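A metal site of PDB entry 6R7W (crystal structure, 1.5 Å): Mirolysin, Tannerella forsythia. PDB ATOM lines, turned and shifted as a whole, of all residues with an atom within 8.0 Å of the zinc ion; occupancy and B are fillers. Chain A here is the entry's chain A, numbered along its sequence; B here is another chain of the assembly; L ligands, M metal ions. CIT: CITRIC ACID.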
ATOM      1  N   GLY A 128     -26.634 -33.868 -32.931  1.00  0.00           N
ATOM      2  CA  GLY A 128     -25.476 -34.417 -33.632  1.00  0.00           C
ATOM      3  C   GLY A 128     -24.360 -34.610 -32.641  1.00  0.00           C
ATOM      4  O   GLY A 128     -24.492 -34.162 -31.489  1.00  0.00           O
ATOM      5  N   TYR A 129     -23.289 -35.323 -33.039  1.00  0.00           N
ATOM      6  CA  TYR A 129     -22.168 -35.472 -32.115  1.00  0.00           C
ATOM      7  C   TYR A 129     -20.874 -35.679 -32.872  1.00  0.00           C
ATOM      8  O   TYR A 129     -20.897 -36.062 -34.047  1.00  0.00           O
ATOM      9  CB  TYR A 129     -22.405 -36.602 -31.082  1.00  0.00           C
ATOM     10  CG  TYR A 129     -22.338 -38.015 -31.598  1.00  0.00           C
ATOM     11  CD1 TYR A 129     -21.139 -38.730 -31.581  1.00  0.00           C
ATOM     12  CD2 TYR A 129     -23.469 -38.652 -32.096  1.00  0.00           C
ATOM     13  CE1 TYR A 129     -21.087 -40.059 -32.010  1.00  0.00           C
ATOM     14  CE2 TYR A 129     -23.426 -39.980 -32.543  1.00  0.00           C
ATOM     15  CZ  TYR A 129     -22.228 -40.664 -32.514  1.00  0.00           C
ATOM     16  OH  TYR A 129     -22.156 -41.983 -32.941  1.00  0.00           O
ATOM     17  N   ALA A 130     -19.746 -35.392 -32.205  1.00  0.00           N
ATOM     18  CA  ALA A 130     -18.433 -35.431 -32.822  1.00  0.00           C
ATOM     19  C   ALA A 130     -17.481 -36.309 -32.015  1.00  0.00           C
ATOM     20  O   ALA A 130     -17.821 -36.765 -30.924  1.00  0.00           O
ATOM     21  CB  ALA A 130     -17.887 -34.005 -32.875  1.00  0.00           C
ATOM     22  N   PHE A 132     -13.503 -35.879 -30.698  1.00  0.00           N
ATOM     23  CA  PHE A 132     -12.461 -34.870 -30.534  1.00  0.00           C
ATOM     24  C   PHE A 132     -11.087 -35.376 -30.983  1.00  0.00           C
ATOM     25  O   PHE A 132     -10.817 -36.607 -30.937  1.00  0.00           O
ATOM     26  CB  PHE A 132     -12.425 -34.449 -29.054  1.00  0.00           C
ATOM     27  CG  PHE A 132     -13.598 -33.594 -28.647  1.00  0.00           C
ATOM     28  CD1 PHE A 132     -14.833 -34.166 -28.362  1.00  0.00           C
ATOM     29  CD2 PHE A 132     -13.512 -32.207 -28.671  1.00  0.00           C
ATOM     30  CE1 PHE A 132     -15.939 -33.370 -28.033  1.00  0.00           C
ATOM     31  CE2 PHE A 132     -14.604 -31.418 -28.293  1.00  0.00           C
ATOM     32  CZ  PHE A 132     -15.813 -32.008 -27.977  1.00  0.00           C
ATOM     33  N   THR A 167     -25.828 -27.247 -36.904  1.00  0.00           N
ATOM     34  CA  THR A 167     -25.430 -28.380 -36.051  1.00  0.00           C
ATOM     35  C   THR A 167     -24.097 -28.903 -36.559  1.00  0.00           C
ATOM     36  O   THR A 167     -23.166 -29.099 -35.778  1.00  0.00           O
ATOM     37  CB  THR A 167     -26.472 -29.486 -36.074  1.00  0.00           C
ATOM     38  OG1 THR A 167     -27.724 -28.965 -35.616  1.00  0.00           O
ATOM     39  CG2 THR A 167     -26.080 -30.657 -35.175  1.00  0.00           C
ATOM     40  N   HIS A 170     -21.179 -26.550 -35.667  1.00  0.00           N
ATOM     41  CA  HIS A 170     -20.829 -26.768 -34.266  1.00  0.00           C
ATOM     42  C   HIS A 170     -20.024 -28.082 -34.089  1.00  0.00           C
ATOM     43  O   HIS A 170     -18.972 -28.071 -33.449  1.00  0.00           O
ATOM     44  CB  HIS A 170     -22.135 -26.771 -33.443  1.00  0.00           C
ATOM     45  CG  HIS A 170     -21.978 -27.031 -31.963  1.00  0.00           C
ATOM     46  ND1 HIS A 170     -22.130 -26.007 -31.041  1.00  0.00           N
ATOM     47  CD2 HIS A 170     -21.832 -28.198 -31.290  1.00  0.00           C
ATOM     48  CE1 HIS A 170     -22.072 -26.588 -29.843  1.00  0.00           C
ATOM     49  NE2 HIS A 170     -21.847 -27.894 -29.944  1.00  0.00           N
ATOM     50  N   GLU A 171     -20.495 -29.190 -34.706  1.00  0.00           N
ATOM     51  CA  GLU A 171     -19.791 -30.475 -34.569  1.00  0.00           C
ATOM     52  C   GLU A 171     -18.466 -30.464 -35.256  1.00  0.00           C
ATOM     53  O   GLU A 171     -17.512 -31.028 -34.697  1.00  0.00           O
ATOM     54  CB  GLU A 171     -20.643 -31.623 -35.126  1.00  0.00           C
ATOM     55  CG  GLU A 171     -21.961 -31.837 -34.404  1.00  0.00           C
ATOM     56  CD  GLU A 171     -21.849 -31.849 -32.895  1.00  0.00           C
ATOM     57  OE1 GLU A 171     -20.969 -32.555 -32.338  1.00  0.00           O
ATOM     58  OE2 GLU A 171     -22.632 -31.125 -32.245  1.00  0.00           O
ATOM     59  N   GLY A 173     -16.652 -27.899 -35.527  1.00  0.00           N
ATOM     60  CA  GLY A 173     -15.863 -27.158 -34.541  1.00  0.00           C
ATOM     61  C   GLY A 173     -15.247 -28.079 -33.498  1.00  0.00           C
ATOM     62  O   GLY A 173     -14.056 -27.988 -33.222  1.00  0.00           O
ATOM     63  N   HIS A 174     -16.045 -28.994 -32.911  1.00  0.00           N
ATOM     64  CA  HIS A 174     -15.522 -29.971 -31.925  1.00  0.00           C
ATOM     65  C   HIS A 174     -14.497 -30.920 -32.564  1.00  0.00           C
ATOM     66  O   HIS A 174     -13.490 -31.215 -31.955  1.00  0.00           O
ATOM     67  CB  HIS A 174     -16.654 -30.818 -31.332  1.00  0.00           C
ATOM     68  CG  HIS A 174     -17.610 -30.115 -30.390  1.00  0.00           C
ATOM     69  ND1 HIS A 174     -17.164 -29.286 -29.359  1.00  0.00           N
ATOM     70  CD2 HIS A 174     -18.946 -30.247 -30.288  1.00  0.00           C
ATOM     71  CE1 HIS A 174     -18.251 -28.938 -28.676  1.00  0.00           C
ATOM     72  NE2 HIS A 174     -19.349 -29.497 -29.187  1.00  0.00           N
ATOM     73  N   LEU A 178     -12.504 -27.479 -30.844  1.00  0.00           N
ATOM     74  CA  LEU A 178     -13.158 -26.438 -30.047  1.00  0.00           C
ATOM     75  C   LEU A 178     -14.044 -27.026 -28.966  1.00  0.00           C
ATOM     76  O   LEU A 178     -14.689 -28.070 -29.176  1.00  0.00           O
ATOM     77  CB  LEU A 178     -13.997 -25.484 -30.917  1.00  0.00           C
ATOM     78  CG  LEU A 178     -13.263 -24.746 -32.032  1.00  0.00           C
ATOM     79  CD1 LEU A 178     -14.198 -23.736 -32.699  1.00  0.00           C
ATOM     80  CD2 LEU A 178     -11.971 -24.058 -31.499  1.00  0.00           C
ATOM     81  N   ARG A 179     -14.071 -26.334 -27.824  1.00  0.00           N
ATOM     82  CA  ARG A 179     -14.953 -26.722 -26.705  1.00  0.00           C
ATOM     83  C   ARG A 179     -16.067 -25.698 -26.543  1.00  0.00           C
ATOM     84  O   ARG A 179     -15.986 -24.572 -27.059  1.00  0.00           O
ATOM     85  CB  ARG A 179     -14.134 -26.822 -25.392  1.00  0.00           C
ATOM     86  CG  ARG A 179     -12.885 -27.748 -25.483  1.00  0.00           C
ATOM     87  CD  ARG A 179     -13.214 -29.112 -26.041  1.00  0.00           C
ATOM     88  NE  ARG A 179     -12.255 -30.168 -25.665  1.00  0.00           N
ATOM     89  CZ  ARG A 179     -11.236 -30.570 -26.406  1.00  0.00           C
ATOM     90  NH1 ARG A 179     -10.979 -29.974 -27.565  1.00  0.00           N
ATOM     91  NH2 ARG A 179     -10.452 -31.559 -26.011  1.00  0.00           N
ATOM     92  N   HIS A 180     -17.121 -26.125 -25.853  1.00  0.00           N
ATOM     93  CA  HIS A 180     -18.244 -25.231 -25.535  1.00  0.00           C
ATOM     94  C   HIS A 180     -17.746 -23.941 -24.937  1.00  0.00           C
ATOM     95  O   HIS A 180     -16.908 -23.942 -24.029  1.00  0.00           O
ATOM     96  CB  HIS A 180     -19.188 -25.918 -24.583  1.00  0.00           C
ATOM     97  CG  HIS A 180     -19.962 -26.974 -25.286  1.00  0.00           C
ATOM     98  ND1 HIS A 180     -20.333 -28.134 -24.644  1.00  0.00           N
ATOM     99  CD2 HIS A 180     -20.344 -27.045 -26.580  1.00  0.00           C
ATOM    100  CE1 HIS A 180     -20.982 -28.851 -25.541  1.00  0.00           C
ATOM    101  NE2 HIS A 180     -20.999 -28.250 -26.734  1.00  0.00           N
ATOM    102  N   ILE A 181     -18.306 -22.832 -25.425  1.00  0.00           N
ATOM    103  CA  ILE A 181     -17.835 -21.502 -25.024  1.00  0.00           C
ATOM    104  C   ILE A 181     -18.006 -21.269 -23.506  1.00  0.00           C
ATOM    105  O   ILE A 181     -17.197 -20.531 -22.929  1.00  0.00           O
ATOM    106  CB  ILE A 181     -18.557 -20.438 -25.902  1.00  0.00           C
ATOM    107  CG1 ILE A 181     -17.941 -19.064 -25.679  1.00  0.00           C
ATOM    108  CG2 ILE A 181     -20.104 -20.419 -25.739  1.00  0.00           C
ATOM    109  CD1 ILE A 181     -18.366 -18.063 -26.778  1.00  0.00           C
ATOM    110  N   TRP A 182     -18.980 -21.917 -22.872  1.00  0.00           N
ATOM    111  CA  TRP A 182     -19.215 -21.719 -21.434  1.00  0.00           C
ATOM    112  C   TRP A 182     -18.302 -22.611 -20.566  1.00  0.00           C
ATOM    113  O   TRP A 182     -18.314 -22.493 -19.338  1.00  0.00           O
ATOM    114  CB  TRP A 182     -20.689 -21.926 -21.070  1.00  0.00           C
ATOM    115  CG  TRP A 182     -21.153 -23.334 -21.177  1.00  0.00           C
ATOM    116  CD1 TRP A 182     -21.212 -24.261 -20.167  1.00  0.00           C
ATOM    117  CD2 TRP A 182     -21.669 -23.976 -22.346  1.00  0.00           C
ATOM    118  NE1 TRP A 182     -21.684 -25.452 -20.652  1.00  0.00           N
ATOM    119  CE2 TRP A 182     -21.967 -25.311 -21.987  1.00  0.00           C
ATOM    120  CE3 TRP A 182     -21.909 -23.550 -23.660  1.00  0.00           C
ATOM    121  CZ2 TRP A 182     -22.525 -26.219 -22.900  1.00  0.00           C
ATOM    122  CZ3 TRP A 182     -22.454 -24.454 -24.567  1.00  0.00           C
ATOM    123  CH2 TRP A 182     -22.762 -25.763 -24.192  1.00  0.00           C
ATOM    124  N   ASP A 184     -18.349 -26.023 -20.032  1.00  0.00           N
ATOM    125  CA  ASP A 184     -18.900 -27.323 -19.563  1.00  0.00           C
ATOM    126  C   ASP A 184     -18.773 -27.455 -18.053  1.00  0.00           C
ATOM    127  O   ASP A 184     -18.322 -28.491 -17.533  1.00  0.00           O
ATOM    128  CB  ASP A 184     -18.164 -28.477 -20.258  1.00  0.00           C
ATOM    129  CG  ASP A 184     -18.407 -28.437 -21.736  1.00  0.00           C
ATOM    130  OD1 ASP A 184     -19.574 -28.516 -22.135  1.00  0.00           O
ATOM    131  OD2 ASP A 184     -17.434 -28.303 -22.486  1.00  0.00           O
ATOM    132  N   TYR A 229     -20.768 -20.092 -32.684  1.00  0.00           N
ATOM    133  CA  TYR A 229     -21.255 -21.426 -33.099  1.00  0.00           C
ATOM    134  C   TYR A 229     -21.101 -22.494 -32.018  1.00  0.00           C
ATOM    135  O   TYR A 229     -21.773 -23.520 -32.093  1.00  0.00           O
ATOM    136  CB  TYR A 229     -20.476 -21.924 -34.361  1.00  0.00           C
ATOM    137  CG  TYR A 229     -20.662 -21.005 -35.554  1.00  0.00           C
ATOM    138  CD1 TYR A 229     -21.942 -20.743 -36.055  1.00  0.00           C
ATOM    139  CD2 TYR A 229     -19.567 -20.491 -36.228  1.00  0.00           C
ATOM    140  CE1 TYR A 229     -22.118 -19.891 -37.155  1.00  0.00           C
ATOM    141  CE2 TYR A 229     -19.722 -19.660 -37.338  1.00  0.00           C
ATOM    142  CZ  TYR A 229     -21.002 -19.373 -37.805  1.00  0.00           C
ATOM    143  OH  TYR A 229     -21.152 -18.556 -38.896  1.00  0.00           O
ATOM    144  N   MET A 230     -20.208 -22.259 -31.019  1.00  0.00           N
ATOM    145  CA  MET A 230     -19.941 -23.234 -29.977  1.00  0.00           C
ATOM    146  C   MET A 230     -20.822 -23.066 -28.764  1.00  0.00           C
ATOM    147  O   MET A 230     -20.534 -23.672 -27.711  1.00  0.00           O
ATOM    148  CB  MET A 230     -18.465 -23.227 -29.617  1.00  0.00           C
ATOM    149  CG  MET A 230     -17.551 -23.555 -30.816  1.00  0.00           C
ATOM    150  SD  MET A 230     -18.056 -24.970 -31.857  1.00  0.00           S
ATOM    151  CE  MET A 230     -18.014 -26.289 -30.707  1.00  0.00           C
ATOM    152  N   ASP A 231     -21.905 -22.271 -28.890  1.00  0.00           N
ATOM    153  CA  ASP A 231     -22.929 -22.194 -27.867  1.00  0.00           C
ATOM    154  C   ASP A 231     -24.077 -23.169 -28.267  1.00  0.00           C
ATOM    155  O   ASP A 231     -23.929 -23.982 -29.204  1.00  0.00           O
ATOM    156  CB  ASP A 231     -23.414 -20.742 -27.649  1.00  0.00           C
ATOM    157  CG  ASP A 231     -23.875 -20.461 -26.224  1.00  0.00           C
ATOM    158  OD1 ASP A 231     -24.404 -21.384 -25.566  1.00  0.00           O
ATOM    159  OD2 ASP A 231     -23.704 -19.315 -25.763  1.00  0.00           O
ATOM    160  N   TYR A 232     -25.238 -23.109 -27.567  1.00  0.00           N
ATOM    161  CA  TYR A 232     -26.366 -24.002 -27.808  1.00  0.00           C
ATOM    162  C   TYR A 232     -27.584 -23.233 -28.347  1.00  0.00           C
ATOM    163  O   TYR A 232     -28.722 -23.713 -28.250  1.00  0.00           O
ATOM    164  CB  TYR A 232     -26.731 -24.749 -26.514  1.00  0.00           C
ATOM    165  CG  TYR A 232     -26.038 -26.069 -26.229  1.00  0.00           C
ATOM    166  CD1 TYR A 232     -25.130 -26.611 -27.132  1.00  0.00           C
ATOM    167  CD2 TYR A 232     -26.334 -26.787 -25.077  1.00  0.00           C
ATOM    168  CE1 TYR A 232     -24.568 -27.876 -26.916  1.00  0.00           C
ATOM    169  CE2 TYR A 232     -25.760 -28.039 -24.844  1.00  0.00           C
ATOM    170  CZ  TYR A 232     -24.878 -28.577 -25.769  1.00  0.00           C
ATOM    171  OH  TYR A 232     -24.337 -29.821 -25.542  1.00  0.00           O
ATOM    172  N   LYS B   1     -24.307 -31.692 -30.210  1.00  0.00           N
ATOM    173  CA  LYS B   1     -25.101 -30.515 -29.830  1.00  0.00           C
ATOM    174  C   LYS B   1     -26.421 -31.001 -29.303  1.00  0.00           C
ATOM    175  O   LYS B   1     -26.997 -31.947 -29.864  1.00  0.00           O
ATOM    176  CB  LYS B   1     -25.291 -29.573 -31.031  1.00  0.00           C
ATOM    177  CG  LYS B   1     -25.691 -28.115 -30.676  1.00  0.00           C
ATOM    178  CD  LYS B   1     -25.639 -27.246 -31.951  1.00  0.00           C
ATOM    179  CE  LYS B   1     -25.922 -25.781 -31.696  1.00  0.00           C
ATOM    180  NZ  LYS B   1     -27.398 -25.513 -31.749  1.00  0.00           N
ATOM    181  N   ARG B   2     -26.873 -30.406 -28.195  1.00  0.00           N
ATOM    182  CA  ARG B   2     -28.177 -30.774 -27.605  1.00  0.00           C
ATOM    183  C   ARG B   2     -29.144 -29.648 -27.787  1.00  0.00           C
ATOM    184  O   ARG B   2     -28.745 -28.480 -27.689  1.00  0.00           O
ATOM    185  CB  ARG B   2     -28.027 -31.052 -26.111  1.00  0.00           C
ATOM    186  CG  ARG B   2     -27.085 -32.190 -25.806  1.00  0.00           C
ATOM    187  CD  ARG B   2     -27.832 -33.478 -25.664  1.00  0.00           C
ATOM    188  NE  ARG B   2     -26.944 -34.630 -25.578  1.00  0.00           N
ATOM    189  CZ  ARG B   2     -27.393 -35.875 -25.532  1.00  0.00           C
ATOM    190  NH1 ARG B   2     -28.697 -36.110 -25.504  1.00  0.00           N
ATOM    191  NH2 ARG B   2     -26.541 -36.892 -25.502  1.00  0.00           N
HETATM  192  C1  CIT L   1     -20.980 -33.748 -29.230  1.00  0.00           C
HETATM  193  O1  CIT L   1     -21.418 -32.863 -29.937  1.00  0.00           O
HETATM  194  O2  CIT L   1     -20.034 -34.543 -29.571  1.00  0.00           O
HETATM  195  C2  CIT L   1     -21.487 -34.006 -27.832  1.00  0.00           C
HETATM  196  C3  CIT L   1     -22.400 -32.888 -27.297  1.00  0.00           C
HETATM  197  O7  CIT L   1     -23.691 -33.004 -27.881  1.00  0.00           O
HETATM  198  C4  CIT L   1     -22.620 -33.038 -25.789  1.00  0.00           C
HETATM  199  C5  CIT L   1     -23.288 -34.331 -25.396  1.00  0.00           C
HETATM  200  O3  CIT L   1     -24.149 -34.882 -26.076  1.00  0.00           O
HETATM  201  O4  CIT L   1     -22.806 -34.858 -24.311  1.00  0.00           O
HETATM  202  C6  CIT L   1     -21.809 -31.521 -27.639  1.00  0.00           C
HETATM  203  O5  CIT L   1     -22.416 -30.662 -28.278  1.00  0.00           O
HETATM  204  O6  CIT L   1     -20.604 -31.384 -27.213  1.00  0.00           O
HETATM  205 ZN    ZN M   1     -21.203 -29.183 -28.526  1.00  0.00          ZN
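Residues that only touch the zinc ion: Tyr 232 (3.95 Å). Four residues have an atom within 4 Å of the zinc ion: His 170, His 174, His 180 and Tyr 232.
The zinc ion is bound by O5 of the ligand (1.9 Å), NE2 of His 174 (2.0 Å), NE2 of His 170 (2.0 Å) and NE2 of His 180 (2.0 Å). Slightly farther from the zinc ion lies O6 of the ligand (2.6 Å).
The backbone carbonyl oxygen (O) of Leu 178 sits at hydrogen-bond distance from a ring nitrogen (ND1) of His 174. A ring nitrogen (ND1) of His 170 lies close to the backbone carbonyl oxygen (O) of Asp 231 (3.3 Å). ND1 of His 170 is in hydrogen-bond range of O of Tyr 229. A ring nitrogen (ND1) of His 180 is in hydrogen-bond range of the side-chain carboxylate (OD1) of Asp 184, 2.6 Å away.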
